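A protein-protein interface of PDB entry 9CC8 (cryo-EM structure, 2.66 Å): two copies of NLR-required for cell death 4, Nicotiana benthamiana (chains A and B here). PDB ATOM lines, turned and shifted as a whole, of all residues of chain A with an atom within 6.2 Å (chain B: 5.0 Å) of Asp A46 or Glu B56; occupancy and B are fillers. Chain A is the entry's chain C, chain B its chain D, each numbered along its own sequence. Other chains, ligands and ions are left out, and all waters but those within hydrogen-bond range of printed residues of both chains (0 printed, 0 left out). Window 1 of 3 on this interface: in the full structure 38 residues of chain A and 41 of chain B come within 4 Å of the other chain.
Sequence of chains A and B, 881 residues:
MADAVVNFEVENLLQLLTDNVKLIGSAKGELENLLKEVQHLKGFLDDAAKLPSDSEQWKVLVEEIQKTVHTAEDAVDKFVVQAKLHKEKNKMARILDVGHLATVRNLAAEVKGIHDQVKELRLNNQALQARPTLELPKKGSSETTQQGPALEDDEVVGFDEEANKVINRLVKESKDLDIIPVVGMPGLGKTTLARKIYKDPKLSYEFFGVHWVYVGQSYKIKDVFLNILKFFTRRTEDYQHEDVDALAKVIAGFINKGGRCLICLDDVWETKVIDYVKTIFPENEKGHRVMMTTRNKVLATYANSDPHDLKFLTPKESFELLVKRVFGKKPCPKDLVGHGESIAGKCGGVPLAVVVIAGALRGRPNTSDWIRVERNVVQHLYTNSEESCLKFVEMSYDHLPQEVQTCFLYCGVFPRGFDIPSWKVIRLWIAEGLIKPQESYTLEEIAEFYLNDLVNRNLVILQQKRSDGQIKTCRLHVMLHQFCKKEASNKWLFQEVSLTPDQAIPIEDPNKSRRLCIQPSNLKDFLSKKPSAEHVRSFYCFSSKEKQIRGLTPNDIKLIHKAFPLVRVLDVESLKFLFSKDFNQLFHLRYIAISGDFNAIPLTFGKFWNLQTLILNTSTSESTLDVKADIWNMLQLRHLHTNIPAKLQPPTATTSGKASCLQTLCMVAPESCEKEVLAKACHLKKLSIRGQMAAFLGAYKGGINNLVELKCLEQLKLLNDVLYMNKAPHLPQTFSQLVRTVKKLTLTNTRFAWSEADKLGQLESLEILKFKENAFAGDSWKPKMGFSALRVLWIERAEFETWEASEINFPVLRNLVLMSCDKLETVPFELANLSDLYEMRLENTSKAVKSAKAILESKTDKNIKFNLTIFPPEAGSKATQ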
ATOM      1  N   GLN A  39      -4.039 -13.762 -16.455  1.00  0.00           N
ATOM      2  CA  GLN A  39      -3.102 -13.243 -17.444  1.00  0.00           C
ATOM      3  C   GLN A  39      -2.076 -14.300 -17.815  1.00  0.00           C
ATOM      4  O   GLN A  39      -1.733 -14.461 -18.992  1.00  0.00           O
ATOM      5  CB  GLN A  39      -2.414 -11.988 -16.906  1.00  0.00           C
ATOM      6  CG  GLN A  39      -2.961 -10.687 -17.471  1.00  0.00           C
ATOM      7  CD  GLN A  39      -4.476 -10.635 -17.461  1.00  0.00           C
ATOM      8  OE1 GLN A  39      -5.094 -10.340 -16.439  1.00  0.00           O
ATOM      9  NE2 GLN A  39      -5.083 -10.922 -18.606  1.00  0.00           N
ATOM     10  N   LEU A  41      -2.562 -17.538 -17.676  1.00  0.00           N
ATOM     11  CA  LEU A  41      -3.277 -18.540 -18.463  1.00  0.00           C
ATOM     12  C   LEU A  41      -3.519 -18.055 -19.888  1.00  0.00           C
ATOM     13  O   LEU A  41      -3.428 -18.835 -20.842  1.00  0.00           O
ATOM     14  CB  LEU A  41      -4.603 -18.888 -17.787  1.00  0.00           C
ATOM     15  CG  LEU A  41      -4.545 -19.598 -16.431  1.00  0.00           C
ATOM     16  CD1 LEU A  41      -5.908 -20.170 -16.089  1.00  0.00           C
ATOM     17  CD2 LEU A  41      -3.493 -20.694 -16.409  1.00  0.00           C
ATOM     18  N   LYS A  42      -3.843 -16.772 -20.054  1.00  0.00           N
ATOM     19  CA  LYS A  42      -4.089 -16.228 -21.385  1.00  0.00           C
ATOM     20  C   LYS A  42      -2.810 -16.180 -22.205  1.00  0.00           C
ATOM     21  O   LYS A  42      -2.831 -16.434 -23.414  1.00  0.00           O
ATOM     22  CB  LYS A  42      -4.706 -14.838 -21.276  1.00  0.00           C
ATOM     23  CG  LYS A  42      -6.113 -14.843 -20.723  1.00  0.00           C
ATOM     24  CD  LYS A  42      -6.622 -13.436 -20.485  1.00  0.00           C
ATOM     25  CE  LYS A  42      -7.066 -12.777 -21.778  1.00  0.00           C
ATOM     26  NZ  LYS A  42      -8.344 -12.032 -21.611  1.00  0.00           N
ATOM     27  N   GLY A  43      -1.689 -15.833 -21.571  1.00  0.00           N
ATOM     28  CA  GLY A  43      -0.414 -15.948 -22.254  1.00  0.00           C
ATOM     29  C   GLY A  43      -0.151 -17.367 -22.714  1.00  0.00           C
ATOM     30  O   GLY A  43       0.311 -17.595 -23.837  1.00  0.00           O
ATOM     31  N   PHE A  44      -0.466 -18.344 -21.862  1.00  0.00           N
ATOM     32  CA  PHE A  44      -0.313 -19.736 -22.267  1.00  0.00           C
ATOM     33  C   PHE A  44      -1.202 -20.063 -23.458  1.00  0.00           C
ATOM     34  O   PHE A  44      -0.794 -20.796 -24.361  1.00  0.00           O
ATOM     35  CB  PHE A  44      -0.639 -20.677 -21.113  1.00  0.00           C
ATOM     36  CG  PHE A  44      -0.775 -22.108 -21.534  1.00  0.00           C
ATOM     37  CD1 PHE A  44       0.343 -22.905 -21.682  1.00  0.00           C
ATOM     38  CD2 PHE A  44      -2.016 -22.649 -21.815  1.00  0.00           C
ATOM     39  CE1 PHE A  44       0.226 -24.216 -22.080  1.00  0.00           C
ATOM     40  CE2 PHE A  44      -2.137 -23.962 -22.216  1.00  0.00           C
ATOM     41  CZ  PHE A  44      -1.014 -24.746 -22.348  1.00  0.00           C
ATOM     42  N   LEU A  45      -2.442 -19.572 -23.452  1.00  0.00           N
ATOM     43  CA  LEU A  45      -3.354 -19.855 -24.557  1.00  0.00           C
ATOM     44  C   LEU A  45      -2.832 -19.267 -25.858  1.00  0.00           C
ATOM     45  O   LEU A  45      -2.888 -19.913 -26.913  1.00  0.00           O
ATOM     46  CB  LEU A  45      -4.743 -19.301 -24.245  1.00  0.00           C
ATOM     47  CG  LEU A  45      -5.523 -20.034 -23.159  1.00  0.00           C
ATOM     48  CD1 LEU A  45      -6.698 -19.199 -22.692  1.00  0.00           C
ATOM     49  CD2 LEU A  45      -5.991 -21.382 -23.670  1.00  0.00           C
ATOM     50  N   ASP A  46      -2.324 -18.037 -25.803  1.00  0.00           N
ATOM     51  CA  ASP A  46      -1.740 -17.427 -26.989  1.00  0.00           C
ATOM     52  C   ASP A  46      -0.558 -18.243 -27.487  1.00  0.00           C
ATOM     53  O   ASP A  46      -0.380 -18.420 -28.698  1.00  0.00           O
ATOM     54  CB  ASP A  46      -1.313 -15.994 -26.682  1.00  0.00           C
ATOM     55  CG  ASP A  46      -2.494 -15.072 -26.463  1.00  0.00           C
ATOM     56  OD1 ASP A  46      -3.448 -15.127 -27.265  1.00  0.00           O
ATOM     57  OD2 ASP A  46      -2.469 -14.295 -25.485  1.00  0.00           O
ATOM     58  N   ASP A  47       0.269 -18.739 -26.566  1.00  0.00           N
ATOM     59  CA  ASP A  47       1.404 -19.567 -26.959  1.00  0.00           C
ATOM     60  C   ASP A  47       0.951 -20.874 -27.595  1.00  0.00           C
ATOM     61  O   ASP A  47       1.503 -21.303 -28.614  1.00  0.00           O
ATOM     62  CB  ASP A  47       2.279 -19.847 -25.746  1.00  0.00           C
ATOM     63  CG  ASP A  47       3.223 -18.719 -25.447  1.00  0.00           C
ATOM     64  OD1 ASP A  47       4.275 -18.988 -24.842  1.00  0.00           O
ATOM     65  OD2 ASP A  47       2.917 -17.569 -25.820  1.00  0.00           O
ATOM     66  N   ALA A  48      -0.045 -21.527 -26.998  1.00  0.00           N
ATOM     67  CA  ALA A  48      -0.527 -22.802 -27.516  1.00  0.00           C
ATOM     68  C   ALA A  48      -1.183 -22.636 -28.875  1.00  0.00           C
ATOM     69  O   ALA A  48      -1.167 -23.568 -29.687  1.00  0.00           O
ATOM     70  CB  ALA A  48      -1.506 -23.431 -26.526  1.00  0.00           C
ATOM     71  N   ALA A  49      -1.767 -21.467 -29.142  1.00  0.00           N
ATOM     72  CA  ALA A  49      -2.300 -21.204 -30.472  1.00  0.00           C
ATOM     73  C   ALA A  49      -1.221 -21.294 -31.542  1.00  0.00           C
ATOM     74  O   ALA A  49      -1.544 -21.487 -32.718  1.00  0.00           O
ATOM     75  CB  ALA A  49      -2.959 -19.827 -30.515  1.00  0.00           C
ATOM     76  N   LYS A  50       0.048 -21.152 -31.161  1.00  0.00           N
ATOM     77  CA  LYS A  50       1.157 -21.278 -32.097  1.00  0.00           C
ATOM     78  C   LYS A  50       1.691 -22.699 -32.176  1.00  0.00           C
ATOM     79  O   LYS A  50       2.235 -23.093 -33.212  1.00  0.00           O
ATOM     80  CB  LYS A  50       2.309 -20.349 -31.696  1.00  0.00           C
ATOM     81  CG  LYS A  50       1.911 -19.085 -30.944  1.00  0.00           C
ATOM     82  CD  LYS A  50       1.136 -18.117 -31.816  1.00  0.00           C
ATOM     83  CE  LYS A  50       2.060 -17.246 -32.652  1.00  0.00           C
ATOM     84  NZ  LYS A  50       3.084 -16.532 -31.839  1.00  0.00           N
ATOM     85  N   LEU A  51       1.555 -23.468 -31.111  1.00  0.00           N
ATOM     86  CA  LEU A  51       2.133 -24.803 -31.062  1.00  0.00           C
ATOM     87  C   LEU A  51       1.269 -25.776 -31.857  1.00  0.00           C
ATOM     88  O   LEU A  51       0.074 -25.903 -31.574  1.00  0.00           O
ATOM     89  CB  LEU A  51       2.249 -25.278 -29.619  1.00  0.00           C
ATOM     90  CG  LEU A  51       3.067 -24.380 -28.692  1.00  0.00           C
ATOM     91  CD1 LEU A  51       2.929 -24.826 -27.250  1.00  0.00           C
ATOM     92  CD2 LEU A  51       4.516 -24.373 -29.111  1.00  0.00           C
ATOM     93  N   GLU A 135       8.371 -21.483 -27.694  1.00  0.00           N
ATOM     94  CA  GLU A 135       7.404 -22.254 -28.448  1.00  0.00           C
ATOM     95  C   GLU A 135       8.226 -23.138 -29.372  1.00  0.00           C
ATOM     96  O   GLU A 135       9.322 -22.756 -29.792  1.00  0.00           O
ATOM     97  CB  GLU A 135       6.432 -21.369 -29.229  1.00  0.00           C
ATOM     98  CG  GLU A 135       5.896 -20.193 -28.439  1.00  0.00           C
ATOM     99  CD  GLU A 135       6.726 -18.950 -28.616  1.00  0.00           C
ATOM    100  OE1 GLU A 135       6.852 -18.481 -29.767  1.00  0.00           O
ATOM    101  OE2 GLU A 135       7.258 -18.446 -27.607  1.00  0.00           O
ATOM    102  N   GLN A 402      -1.273 -10.738 -35.721  1.00  0.00           N
ATOM    103  CA  GLN A 402      -2.191 -11.411 -34.807  1.00  0.00           C
ATOM    104  C   GLN A 402      -3.539 -10.700 -34.750  1.00  0.00           C
ATOM    105  O   GLN A 402      -4.592 -11.350 -34.772  1.00  0.00           O
ATOM    106  CB  GLN A 402      -1.555 -11.500 -33.419  1.00  0.00           C
ATOM    107  CG  GLN A 402      -1.809 -12.805 -32.679  1.00  0.00           C
ATOM    108  CD  GLN A 402      -3.023 -12.747 -31.782  1.00  0.00           C
ATOM    109  OE1 GLN A 402      -3.161 -11.838 -30.964  1.00  0.00           O
ATOM    110  NE2 GLN A 402      -3.912 -13.723 -31.925  1.00  0.00           N
ATOM    111  N   ASP B  54       9.745 -15.195 -27.590  1.00  0.00           N
ATOM    112  CA  ASP B  54       8.566 -15.155 -28.441  1.00  0.00           C
ATOM    113  C   ASP B  54       7.321 -15.657 -27.725  1.00  0.00           C
ATOM    114  O   ASP B  54       6.269 -15.787 -28.360  1.00  0.00           O
ATOM    115  CB  ASP B  54       8.795 -15.985 -29.710  1.00  0.00           C
ATOM    116  CG  ASP B  54       9.439 -17.321 -29.419  1.00  0.00           C
ATOM    117  OD1 ASP B  54       9.648 -17.624 -28.229  1.00  0.00           O
ATOM    118  OD2 ASP B  54       9.731 -18.069 -30.374  1.00  0.00           O
ATOM    119  N   SER B  55       7.412 -15.943 -26.429  1.00  0.00           N
ATOM    120  CA  SER B  55       6.316 -16.524 -25.672  1.00  0.00           C
ATOM    121  C   SER B  55       5.541 -15.438 -24.942  1.00  0.00           C
ATOM    122  O   SER B  55       6.132 -14.595 -24.262  1.00  0.00           O
ATOM    123  CB  SER B  55       6.853 -17.550 -24.677  1.00  0.00           C
ATOM    124  OG  SER B  55       7.585 -18.561 -25.342  1.00  0.00           O
ATOM    125  N   GLU B  56       4.216 -15.461 -25.087  1.00  0.00           N
ATOM    126  CA  GLU B  56       3.381 -14.512 -24.363  1.00  0.00           C
ATOM    127  C   GLU B  56       3.341 -14.827 -22.877  1.00  0.00           C
ATOM    128  O   GLU B  56       3.239 -13.912 -22.053  1.00  0.00           O
ATOM    129  CB  GLU B  56       1.970 -14.510 -24.943  1.00  0.00           C
ATOM    130  CG  GLU B  56       1.915 -14.104 -26.398  1.00  0.00           C
ATOM    131  CD  GLU B  56       2.417 -12.695 -26.627  1.00  0.00           C
ATOM    132  OE1 GLU B  56       1.936 -11.772 -25.935  1.00  0.00           O
ATOM    133  OE2 GLU B  56       3.295 -12.513 -27.494  1.00  0.00           O
ATOM    134  N   GLN B  57       3.410 -16.110 -22.516  1.00  0.00           N
ATOM    135  CA  GLN B  57       3.496 -16.479 -21.109  1.00  0.00           C
ATOM    136  C   GLN B  57       4.806 -15.998 -20.499  1.00  0.00           C
ATOM    137  O   GLN B  57       4.836 -15.554 -19.346  1.00  0.00           O
ATOM    138  CB  GLN B  57       3.356 -17.990 -20.954  1.00  0.00           C
ATOM    139  CG  GLN B  57       2.958 -18.420 -19.558  1.00  0.00           C
ATOM    140  CD  GLN B  57       2.565 -19.877 -19.488  1.00  0.00           C
ATOM    141  OE1 GLN B  57       2.849 -20.656 -20.397  1.00  0.00           O
ATOM    142  NE2 GLN B  57       1.905 -20.255 -18.402  1.00  0.00           N
ATOM    143  N   TRP B  58       5.899 -16.080 -21.256  1.00  0.00           N
ATOM    144  CA  TRP B  58       7.163 -15.532 -20.784  1.00  0.00           C
ATOM    145  C   TRP B  58       7.062 -14.029 -20.574  1.00  0.00           C
ATOM    146  O   TRP B  58       7.566 -13.498 -19.578  1.00  0.00           O
ATOM    147  CB  TRP B  58       8.273 -15.852 -21.779  1.00  0.00           C
ATOM    148  CG  TRP B  58       9.607 -15.371 -21.342  1.00  0.00           C
ATOM    149  CD1 TRP B  58      10.286 -14.294 -21.818  1.00  0.00           C
ATOM    150  CD2 TRP B  58      10.429 -15.947 -20.327  1.00  0.00           C
ATOM    151  NE1 TRP B  58      11.487 -14.165 -21.168  1.00  0.00           N
ATOM    152  CE2 TRP B  58      11.598 -15.171 -20.246  1.00  0.00           C
ATOM    153  CE3 TRP B  58      10.293 -17.050 -19.485  1.00  0.00           C
ATOM    154  CZ2 TRP B  58      12.624 -15.463 -19.355  1.00  0.00           C
ATOM    155  CZ3 TRP B  58      11.305 -17.336 -18.607  1.00  0.00           C
ATOM    156  CH2 TRP B  58      12.457 -16.548 -18.544  1.00  0.00           C
ATOM    157  N   LYS B  59       6.419 -13.328 -21.509  1.00  0.00           N
ATOM    158  CA  LYS B  59       6.214 -11.893 -21.357  1.00  0.00           C
ATOM    159  C   LYS B  59       5.406 -11.589 -20.105  1.00  0.00           C
ATOM    160  O   LYS B  59       5.721 -10.650 -19.365  1.00  0.00           O
ATOM    161  CB  LYS B  59       5.503 -11.341 -22.590  1.00  0.00           C
ATOM    162  CG  LYS B  59       6.424 -11.021 -23.753  1.00  0.00           C
ATOM    163  CD  LYS B  59       5.641 -10.652 -25.007  1.00  0.00           C
ATOM    164  CE  LYS B  59       4.654  -9.513 -24.760  1.00  0.00           C
ATOM    165  NZ  LYS B  59       5.249  -8.393 -23.978  1.00  0.00           N
ATOM    166  N   VAL B  60       4.358 -12.372 -19.854  1.00  0.00           N
ATOM    167  CA  VAL B  60       3.531 -12.149 -18.674  1.00  0.00           C
ATOM    168  C   VAL B  60       4.344 -12.372 -17.408  1.00  0.00           C
ATOM    169  O   VAL B  60       4.250 -11.601 -16.448  1.00  0.00           O
ATOM    170  CB  VAL B  60       2.290 -13.061 -18.719  1.00  0.00           C
ATOM    171  CG1 VAL B  60       1.460 -12.896 -17.458  1.00  0.00           C
ATOM    172  CG2 VAL B  60       1.458 -12.761 -19.947  1.00  0.00           C
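Of the printed residues of chain B, Phe A44 touches Gln B57 (3.6 Å).
Of the printed residues of chain B, Asp A47 touches Ser B55 (3.0 Å), Glu B56 (2.6 Å) and Gln B57 (3.6 Å).
Of the printed residues of chain A, Asp B54 touches Glu A135 (2.6 Å).
Printed residues of chain A within 4 Å of Ser B55: Asp A47 (3.0 Å) and Glu A135 (2.3 Å).
Glu B56 touches just these residues of chain A: Gly A43, Asp A46 and Asp A47.
Of the printed residues of chain A, Gln B57 touches Gly A43, Phe A44 and Asp A47.
The nearest printed residue of chain B that does not touch Asp A46 is Gln B57 (6.3 Å).
The nearest residue of chain A that does not touch Glu B56 is Glu A135 (5.0 Å).
No position is printed for both chains.
Of the 10 pairs that touch across the chains among the printed residues, none has its exchanged pair printed and touching as well.
Of the 7 printed residues of chain B, 5 touch a printed residue of chain A.
Printed residues of chain A that touch a printed residue of chain B: Gln A39, Gly A43, Phe A44, Asp A46, Asp A47 and Glu A135.
Hydrophobic or aromatic side chains of chain A within 4 Å of the printed part of chain B: Phe A44.
CG2 of Val B60 touches O of Gln A39, 3.7 Å away.
Gly A43 touches Glu B56 (O to CB, 3.7 Å).
Gln B57 touches Gly A43.
Gln B57 touches Phe A44 (OE1 to CB, 3.6 Å).
Asp A46 touches Glu B56.
Gln B57 touches Asp A47.
The side-chain carboxylate (OE2) of Glu A135 lies within hydrogen-bond range of the backbone NH (N) of Ser B55 (2.8 Å).
OE2 of Glu A135 lies close to OD1 of Asp B54 (2.6 Å).
The side-chain carboxylate (OD1) of Asp A47 sits close to the side-chain hydroxyl (OG) of Ser B55 (3.4 Å).
The side-chain carboxylate of Asp A47 lies within hydrogen-bond range of the backbone NH of Glu B56.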
